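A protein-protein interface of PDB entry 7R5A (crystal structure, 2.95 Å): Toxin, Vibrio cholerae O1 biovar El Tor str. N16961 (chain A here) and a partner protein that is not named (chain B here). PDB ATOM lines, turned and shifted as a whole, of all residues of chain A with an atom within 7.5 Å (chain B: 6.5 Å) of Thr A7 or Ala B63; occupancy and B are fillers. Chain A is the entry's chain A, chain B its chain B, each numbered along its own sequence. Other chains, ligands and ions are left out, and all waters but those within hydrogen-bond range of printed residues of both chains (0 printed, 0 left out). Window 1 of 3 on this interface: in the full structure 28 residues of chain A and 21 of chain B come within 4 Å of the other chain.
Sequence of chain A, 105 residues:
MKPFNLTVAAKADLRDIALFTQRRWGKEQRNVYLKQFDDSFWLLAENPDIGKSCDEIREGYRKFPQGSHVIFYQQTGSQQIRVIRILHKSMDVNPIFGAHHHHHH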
ATOM      1  N   PHE A   4      34.605  34.499  13.319  1.00  0.00           N
ATOM      2  CA  PHE A   4      33.482  33.575  13.313  1.00  0.00           C
ATOM      3  C   PHE A   4      32.406  34.141  12.401  1.00  0.00           C
ATOM      4  O   PHE A   4      32.282  35.359  12.245  1.00  0.00           O
ATOM      5  CB  PHE A   4      32.929  33.342  14.726  1.00  0.00           C
ATOM      6  CG  PHE A   4      32.302  34.562  15.342  1.00  0.00           C
ATOM      7  CD1 PHE A   4      33.072  35.479  16.038  1.00  0.00           C
ATOM      8  CD2 PHE A   4      30.939  34.788  15.227  1.00  0.00           C
ATOM      9  CE1 PHE A   4      32.495  36.601  16.604  1.00  0.00           C
ATOM     10  CE2 PHE A   4      30.357  35.909  15.789  1.00  0.00           C
ATOM     11  CZ  PHE A   4      31.136  36.815  16.480  1.00  0.00           C
ATOM     12  N   ASN A   5      31.629  33.247  11.796  1.00  0.00           N
ATOM     13  CA  ASN A   5      30.558  33.667  10.907  1.00  0.00           C
ATOM     14  C   ASN A   5      29.423  32.660  10.991  1.00  0.00           C
ATOM     15  O   ASN A   5      29.658  31.452  11.081  1.00  0.00           O
ATOM     16  CB  ASN A   5      31.053  33.806   9.462  1.00  0.00           C
ATOM     17  CG  ASN A   5      30.135  34.667   8.617  1.00  0.00           C
ATOM     18  OD1 ASN A   5      29.239  35.333   9.137  1.00  0.00           O
ATOM     19  ND2 ASN A   5      30.357  34.663   7.307  1.00  0.00           N
ATOM     20  N   LEU A   6      28.197  33.167  10.968  1.00  0.00           N
ATOM     21  CA  LEU A   6      27.000  32.348  11.070  1.00  0.00           C
ATOM     22  C   LEU A   6      26.381  32.139   9.694  1.00  0.00           C
ATOM     23  O   LEU A   6      26.644  32.882   8.745  1.00  0.00           O
ATOM     24  CB  LEU A   6      25.972  32.993  12.007  1.00  0.00           C
ATOM     25  CG  LEU A   6      26.199  32.967  13.522  1.00  0.00           C
ATOM     26  CD1 LEU A   6      27.344  33.875  13.948  1.00  0.00           C
ATOM     27  CD2 LEU A   6      24.917  33.350  14.247  1.00  0.00           C
ATOM     28  N   THR A   7      25.549  31.108   9.597  1.00  0.00           N
ATOM     29  CA  THR A   7      24.805  30.839   8.379  1.00  0.00           C
ATOM     30  C   THR A   7      23.449  31.538   8.425  1.00  0.00           C
ATOM     31  O   THR A   7      23.044  32.103   9.444  1.00  0.00           O
ATOM     32  CB  THR A   7      24.618  29.336   8.180  1.00  0.00           C
ATOM     33  OG1 THR A   7      23.895  28.793   9.291  1.00  0.00           O
ATOM     34  CG2 THR A   7      25.966  28.641   8.075  1.00  0.00           C
ATOM     35  N   VAL A   8      22.744  31.500   7.293  1.00  0.00           N
ATOM     36  CA  VAL A   8      21.406  32.081   7.240  1.00  0.00           C
ATOM     37  C   VAL A   8      20.478  31.356   8.205  1.00  0.00           C
ATOM     38  O   VAL A   8      19.652  31.978   8.884  1.00  0.00           O
ATOM     39  CB  VAL A   8      20.863  32.056   5.798  1.00  0.00           C
ATOM     40  CG1 VAL A   8      19.445  32.607   5.748  1.00  0.00           C
ATOM     41  CG2 VAL A   8      21.773  32.854   4.876  1.00  0.00           C
ATOM     42  N   ALA A   9      20.617  30.032   8.303  1.00  0.00           N
ATOM     43  CA  ALA A   9      19.806  29.278   9.251  1.00  0.00           C
ATOM     44  C   ALA A   9      20.176  29.619  10.688  1.00  0.00           C
ATOM     45  O   ALA A   9      19.296  29.752  11.546  1.00  0.00           O
ATOM     46  CB  ALA A   9      19.958  27.779   8.997  1.00  0.00           C
ATOM     47  N   ALA A  10      21.472  29.773  10.972  1.00  0.00           N
ATOM     48  CA  ALA A  10      21.892  30.126  12.325  1.00  0.00           C
ATOM     49  C   ALA A  10      21.417  31.524  12.700  1.00  0.00           C
ATOM     50  O   ALA A  10      20.985  31.758  13.837  1.00  0.00           O
ATOM     51  CB  ALA A  10      23.412  30.020  12.448  1.00  0.00           C
ATOM     52  N   LYS A  11      21.477  32.465  11.756  1.00  0.00           N
ATOM     53  CA  LYS A  11      20.979  33.810  12.020  1.00  0.00           C
ATOM     54  C   LYS A  11      19.468  33.805  12.215  1.00  0.00           C
ATOM     55  O   LYS A  11      18.945  34.535  13.064  1.00  0.00           O
ATOM     56  CB  LYS A  11      21.380  34.749  10.883  1.00  0.00           C
ATOM     57  CG  LYS A  11      21.155  36.222  11.185  1.00  0.00           C
ATOM     58  CD  LYS A  11      21.683  37.104  10.062  1.00  0.00           C
ATOM     59  CE  LYS A  11      21.492  38.580  10.372  1.00  0.00           C
ATOM     60  NZ  LYS A  11      22.036  39.454   9.296  1.00  0.00           N
ATOM     61  N   ALA A  12      18.751  32.976  11.450  1.00  0.00           N
ATOM     62  CA  ALA A  12      17.309  32.854  11.647  1.00  0.00           C
ATOM     63  C   ALA A  12      16.986  32.267  13.017  1.00  0.00           C
ATOM     64  O   ALA A  12      16.038  32.707  13.676  1.00  0.00           O
ATOM     65  CB  ALA A  12      16.696  32.001  10.535  1.00  0.00           C
ATOM     66  N   ASP A  13      17.762  31.276  13.461  1.00  0.00           N
ATOM     67  CA  ASP A  13      17.562  30.708  14.793  1.00  0.00           C
ATOM     68  C   ASP A  13      17.813  31.752  15.872  1.00  0.00           C
ATOM     69  O   ASP A  13      17.048  31.862  16.840  1.00  0.00           O
ATOM     70  CB  ASP A  13      18.477  29.503  14.997  1.00  0.00           C
ATOM     71  CG  ASP A  13      18.198  28.385  14.016  1.00  0.00           C
ATOM     72  OD1 ASP A  13      17.027  28.216  13.614  1.00  0.00           O
ATOM     73  OD2 ASP A  13      19.155  27.671  13.649  1.00  0.00           O
ATOM     74  N   PHE A  72      25.847  24.564  17.456  1.00  0.00           N
ATOM     75  CA  PHE A  72      26.607  23.603  16.668  1.00  0.00           C
ATOM     76  C   PHE A  72      27.526  24.369  15.728  1.00  0.00           C
ATOM     77  O   PHE A  72      27.075  25.266  15.007  1.00  0.00           O
ATOM     78  CB  PHE A  72      25.679  22.674  15.883  1.00  0.00           C
ATOM     79  CG  PHE A  72      24.938  21.689  16.746  1.00  0.00           C
ATOM     80  CD1 PHE A  72      23.757  22.046  17.377  1.00  0.00           C
ATOM     81  CD2 PHE A  72      25.428  20.405  16.930  1.00  0.00           C
ATOM     82  CE1 PHE A  72      23.076  21.142  18.171  1.00  0.00           C
ATOM     83  CE2 PHE A  72      24.752  19.496  17.723  1.00  0.00           C
ATOM     84  CZ  PHE A  72      23.575  19.865  18.344  1.00  0.00           C
ATOM     85  N   GLN A  74      31.448  24.171  13.334  1.00  0.00           N
ATOM     86  CA  GLN A  74      32.554  23.413  12.771  1.00  0.00           C
ATOM     87  C   GLN A  74      33.800  24.284  12.723  1.00  0.00           C
ATOM     88  O   GLN A  74      33.740  25.457  12.341  1.00  0.00           O
ATOM     89  CB  GLN A  74      32.215  22.877  11.375  1.00  0.00           C
ATOM     90  CG  GLN A  74      31.698  23.915  10.396  1.00  0.00           C
ATOM     91  CD  GLN A  74      31.236  23.292   9.092  1.00  0.00           C
ATOM     92  OE1 GLN A  74      31.062  22.076   9.000  1.00  0.00           O
ATOM     93  NE2 GLN A  74      31.031  24.124   8.076  1.00  0.00           N
ATOM     94  N   ARG A  82      32.782  28.191  12.380  1.00  0.00           N
ATOM     95  CA  ARG A  82      31.575  28.510  11.629  1.00  0.00           C
ATOM     96  C   ARG A  82      30.380  27.957  12.389  1.00  0.00           C
ATOM     97  O   ARG A  82      30.271  26.738  12.574  1.00  0.00           O
ATOM     98  CB  ARG A  82      31.637  27.920  10.220  1.00  0.00           C
ATOM     99  CG  ARG A  82      30.544  28.403   9.283  1.00  0.00           C
ATOM    100  CD  ARG A  82      30.433  27.495   8.069  1.00  0.00           C
ATOM    101  NE  ARG A  82      29.667  28.108   6.987  1.00  0.00           N
ATOM    102  CZ  ARG A  82      29.245  27.456   5.910  1.00  0.00           C
ATOM    103  NH1 ARG A  82      29.505  26.162   5.772  1.00  0.00           N
ATOM    104  NH2 ARG A  82      28.556  28.094   4.973  1.00  0.00           N
ATOM    105  N   VAL A  83      29.497  28.848  12.833  1.00  0.00           N
ATOM    106  CA  VAL A  83      28.296  28.468  13.570  1.00  0.00           C
ATOM    107  C   VAL A  83      27.204  28.126  12.565  1.00  0.00           C
ATOM    108  O   VAL A  83      26.825  28.965  11.742  1.00  0.00           O
ATOM    109  CB  VAL A  83      27.840  29.595  14.508  1.00  0.00           C
ATOM    110  CG1 VAL A  83      26.522  29.231  15.177  1.00  0.00           C
ATOM    111  CG2 VAL A  83      28.912  29.893  15.546  1.00  0.00           C
ATOM    112  N   ILE A  84      26.688  26.902  12.635  1.00  0.00           N
ATOM    113  CA  ILE A  84      25.745  26.403  11.644  1.00  0.00           C
ATOM    114  C   ILE A  84      24.314  26.397  12.169  1.00  0.00           C
ATOM    115  O   ILE A  84      23.385  26.746  11.441  1.00  0.00           O
ATOM    116  CB  ILE A  84      26.179  24.998  11.174  1.00  0.00           C
ATOM    117  CG1 ILE A  84      27.519  25.090  10.443  1.00  0.00           C
ATOM    118  CG2 ILE A  84      25.115  24.367  10.289  1.00  0.00           C
ATOM    119  CD1 ILE A  84      27.929  23.819   9.760  1.00  0.00           C
ATOM    120  N   ARG A  85      24.117  26.018  13.429  1.00  0.00           N
ATOM    121  CA  ARG A  85      22.778  25.899  13.986  1.00  0.00           C
ATOM    122  C   ARG A  85      22.792  26.281  15.458  1.00  0.00           C
ATOM    123  O   ARG A  85      23.787  26.080  16.160  1.00  0.00           O
ATOM    124  CB  ARG A  85      22.229  24.476  13.822  1.00  0.00           C
ATOM    125  CG  ARG A  85      21.589  24.201  12.473  1.00  0.00           C
ATOM    126  CD  ARG A  85      20.365  25.073  12.287  1.00  0.00           C
ATOM    127  NE  ARG A  85      19.434  24.522  11.308  1.00  0.00           N
ATOM    128  CZ  ARG A  85      18.204  24.985  11.118  1.00  0.00           C
ATOM    129  NH1 ARG A  85      17.762  26.003  11.844  1.00  0.00           N
ATOM    130  NH2 ARG A  85      17.415  24.431  10.208  1.00  0.00           N
ATOM    131  N   ILE A  86      21.686  26.857  15.914  1.00  0.00           N
ATOM    132  CA  ILE A  86      21.508  27.204  17.348  1.00  0.00           C
ATOM    133  C   ILE A  86      20.143  26.645  17.722  1.00  0.00           C
ATOM    134  O   ILE A  86      19.185  27.393  17.736  1.00  0.00           O
ATOM    135  CB  ILE A  86      21.584  28.718  17.584  1.00  0.00           C
ATOM    136  CG1 ILE A  86      22.921  29.292  17.128  1.00  0.00           C
ATOM    137  CG2 ILE A  86      21.333  29.029  19.041  1.00  0.00           C
ATOM    138  CD1 ILE A  86      23.065  30.757  17.400  1.00  0.00           C
ATOM    139  N   GLU B  56      20.689  21.256   6.321  1.00  0.00           N
ATOM    140  CA  GLU B  56      20.005  22.424   5.781  1.00  0.00           C
ATOM    141  C   GLU B  56      20.579  23.731   6.312  1.00  0.00           C
ATOM    142  O   GLU B  56      20.400  24.774   5.674  1.00  0.00           O
ATOM    143  CB  GLU B  56      18.508  22.346   6.089  1.00  0.00           C
ATOM    144  CG  GLU B  56      17.800  21.202   5.385  1.00  0.00           C
ATOM    145  CD  GLU B  56      16.322  21.134   5.720  1.00  0.00           C
ATOM    146  OE1 GLU B  56      15.889  21.835   6.659  1.00  0.00           O
ATOM    147  OE2 GLU B  56      15.594  20.381   5.040  1.00  0.00           O
ATOM    148  N   GLY B  57      21.257  23.702   7.457  1.00  0.00           N
ATOM    149  CA  GLY B  57      21.920  24.891   7.949  1.00  0.00           C
ATOM    150  C   GLY B  57      23.255  25.140   7.280  1.00  0.00           C
ATOM    151  O   GLY B  57      23.620  26.291   7.020  1.00  0.00           O
ATOM    152  N   GLU B  58      23.994  24.068   6.988  1.00  0.00           N
ATOM    153  CA  GLU B  58      25.327  24.233   6.421  1.00  0.00           C
ATOM    154  C   GLU B  58      25.292  24.486   4.920  1.00  0.00           C
ATOM    155  O   GLU B  58      26.168  25.188   4.401  1.00  0.00           O
ATOM    156  CB  GLU B  58      26.196  23.009   6.727  1.00  0.00           C
ATOM    157  CG  GLU B  58      25.796  21.733   6.005  1.00  0.00           C
ATOM    158  CD  GLU B  58      26.818  20.627   6.185  1.00  0.00           C
ATOM    159  OE1 GLU B  58      27.895  20.903   6.752  1.00  0.00           O
ATOM    160  OE2 GLU B  58      26.547  19.483   5.765  1.00  0.00           O
ATOM    161  N   GLN B  59      24.310  23.940   4.205  1.00  0.00           N
ATOM    162  CA  GLN B  59      24.211  24.200   2.774  1.00  0.00           C
ATOM    163  C   GLN B  59      23.422  25.467   2.465  1.00  0.00           C
ATOM    164  O   GLN B  59      23.112  25.721   1.297  1.00  0.00           O
ATOM    165  CB  GLN B  59      23.605  22.997   2.044  1.00  0.00           C
ATOM    166  CG  GLN B  59      22.137  22.729   2.307  1.00  0.00           C
ATOM    167  CD  GLN B  59      21.649  21.489   1.577  1.00  0.00           C
ATOM    168  OE1 GLN B  59      22.448  20.719   1.041  1.00  0.00           O
ATOM    169  NE2 GLN B  59      20.337  21.293   1.552  1.00  0.00           N
ATOM    170  N   SER B  60      23.096  26.263   3.479  1.00  0.00           N
ATOM    171  CA  SER B  60      22.568  27.600   3.269  1.00  0.00           C
ATOM    172  C   SER B  60      23.717  28.602   3.196  1.00  0.00           C
ATOM    173  O   SER B  60      24.879  28.277   3.450  1.00  0.00           O
ATOM    174  CB  SER B  60      21.590  27.984   4.380  1.00  0.00           C
ATOM    175  OG  SER B  60      22.265  28.223   5.604  1.00  0.00           O
ATOM    176  N   GLY B  61      23.399  29.860   2.947  1.00  0.00           N
ATOM    177  CA  GLY B  61      24.513  30.803   2.782  1.00  0.00           C
ATOM    178  C   GLY B  61      25.072  31.316   4.086  1.00  0.00           C
ATOM    179  O   GLY B  61      24.385  31.211   5.096  1.00  0.00           O
ATOM    180  N   ASP B  62      26.303  31.828   4.044  1.00  0.00           N
ATOM    181  CA  ASP B  62      26.924  32.489   5.214  1.00  0.00           C
ATOM    182  C   ASP B  62      26.148  33.790   5.370  1.00  0.00           C
ATOM    183  O   ASP B  62      25.894  34.416   4.348  1.00  0.00           O
ATOM    184  CB  ASP B  62      28.373  32.862   4.916  1.00  0.00           C
ATOM    185  CG  ASP B  62      29.396  31.992   5.616  1.00  0.00           C
ATOM    186  OD1 ASP B  62      29.247  30.771   5.567  1.00  0.00           O
ATOM    187  OD2 ASP B  62      30.341  32.553   6.182  1.00  0.00           O
ATOM    188  N   ALA B  63      25.773  34.183   6.582  1.00  0.00           N
ATOM    189  CA  ALA B  63      24.992  35.429   6.707  1.00  0.00           C
ATOM    190  C   ALA B  63      25.868  36.524   7.299  1.00  0.00           C
ATOM    191  O   ALA B  63      26.714  36.210   8.121  1.00  0.00           O
ATOM    192  CB  ALA B  63      23.783  35.183   7.554  1.00  0.00           C
ATOM    193  N   ASP B  64      25.684  37.759   6.851  1.00  0.00           N
ATOM    194  CA  ASP B  64      26.462  38.867   7.396  1.00  0.00           C
ATOM    195  C   ASP B  64      25.962  39.177   8.801  1.00  0.00           C
ATOM    196  O   ASP B  64      24.849  39.683   8.972  1.00  0.00           O
ATOM    197  CB  ASP B  64      26.341  40.088   6.489  1.00  0.00           C
ATOM    198  CG  ASP B  64      27.511  41.041   6.632  1.00  0.00           C
ATOM    199  OD1 ASP B  64      27.577  41.757   7.654  1.00  0.00           O
ATOM    200  OD2 ASP B  64      28.370  41.067   5.726  1.00  0.00           O
ATOM    201  N   TYR B  65      26.773  38.873   9.812  1.00  0.00           N
ATOM    202  CA  TYR B  65      26.366  39.012  11.202  1.00  0.00           C
ATOM    203  C   TYR B  65      27.282  39.979  11.938  1.00  0.00           C
ATOM    204  O   TYR B  65      28.509  39.869  11.859  1.00  0.00           O
ATOM    205  CB  TYR B  65      26.361  37.661  11.925  1.00  0.00           C
ATOM    206  CG  TYR B  65      26.145  37.785  13.420  1.00  0.00           C
ATOM    207  CD1 TYR B  65      24.876  38.003  13.943  1.00  0.00           C
ATOM    208  CD2 TYR B  65      27.210  37.693  14.308  1.00  0.00           C
ATOM    209  CE1 TYR B  65      24.674  38.122  15.305  1.00  0.00           C
ATOM    210  CE2 TYR B  65      27.018  37.810  15.670  1.00  0.00           C
ATOM    211  CZ  TYR B  65      25.749  38.025  16.163  1.00  0.00           C
ATOM    212  OH  TYR B  65      25.554  38.142  17.520  1.00  0.00           O
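The backbone carbonyl oxygen (O) of Ala B63 lies close to the side-chain amide oxygen (OD1) of Asn A5, at 2.9 Å. The backbone NH (N) of Ala B63 sits at hydrogen-bond distance from the backbone carbonyl oxygen (O) of Leu A6, at 2.7 Å. The backbone carbonyl oxygen (O) of Gly B57 sits at hydrogen-bond distance from the side-chain hydroxyl (OG1) of Thr A7. The backbone carbonyl oxygen (O) of Gly B61 is in hydrogen-bond range of the backbone NH (N) of Val A8 (2.8 Å). The side-chain amino group (NZ) of Lys A11 lies within hydrogen-bond range of the backbone carbonyl oxygen (O) of Asp B64. NH2 of Arg A82 lies within salt-bridge range of OD1 of Asp B62 (2.8 Å). ND2 of Asn A5 lies close to OD2 of Asp B62 (2.4 Å).
O of Asn A5 lies within hydrogen-bond range of N of Val A83 (3.1 Å). N of Ala A10 sits at hydrogen-bond distance from OG1 of Thr A7 (3.1 Å). N of Thr A7 lies within hydrogen-bond range of O of Val A83. O of Ile A84 sits at hydrogen-bond distance from OG1 of Thr A7. O of Gln A74 sits at hydrogen-bond distance from N of Arg A82, 2.9 Å away. O of Gly B57 sits at hydrogen-bond distance from OG of Ser B60 (2.8 Å).
Thr A7 touches Ser B60. O of Gly B61 touches CA of Thr A7, at 3.3 Å. Thr A7 touches Ala B63 (O to CB, 3.7 Å). OG of Ser B60 touches N of Val A8 (3.7 Å). OG of Ser B60 touches N of Ala A9, at 3.6 Å. Ala B63 touches Lys A11. O of Glu B58 touches NH1 of Arg A82, at 3.7 Å. O of Ser B60 touches NH2 of Arg A82, 3.98 Å away. Gly B57 touches Ile A84 (C to CG2, 3.6 Å). Ile A84 touches Glu B58.
Of the printed residues of chain B, Leu A6 touches Asp B62 (3.5 Å), Ala B63 (2.7 Å) and Tyr B65 (3.8 Å). Of chain B, only Gly B57 (3.4 Å), Ser B60 (3.7 Å), Gly B61 (3.3 Å) and Ala B63 (3.7 Å) come within 4 Å of Thr A7. Of the printed residues of chain B, Val A8 touches Ser B60 (3.7 Å), Gly B61 (2.8 Å) and Ala B63 (3.8 Å). Asp A13 touches none of the printed residues of chain B. Arg A85 touches none of the printed residues of chain B. The nearest residue of chain B that does not touch Thr A7 is Asp B62 (4.2 Å).
Hydrophobic or aromatic side chains of chain A that line the printed part of chain B: Phe A4, Leu A6, Val A8, Ala A9 and Ile A84. Printed residues of chain B that touch a printed residue of chain A: Gly B57, Glu B58, Ser B60, Gly B61, Asp B62, Ala B63, Asp B64 and Tyr B65. Along chain B the printed residues that touch a printed residue of chain A span positions 57 to 65. Among the printed residues, 22 pairs touch across the chains. Among the printed residues, Asp or Glu carboxylates within 4 Å of a Lys or Arg side-chain nitrogen of the other chain: Arg A82 with Asp B62.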
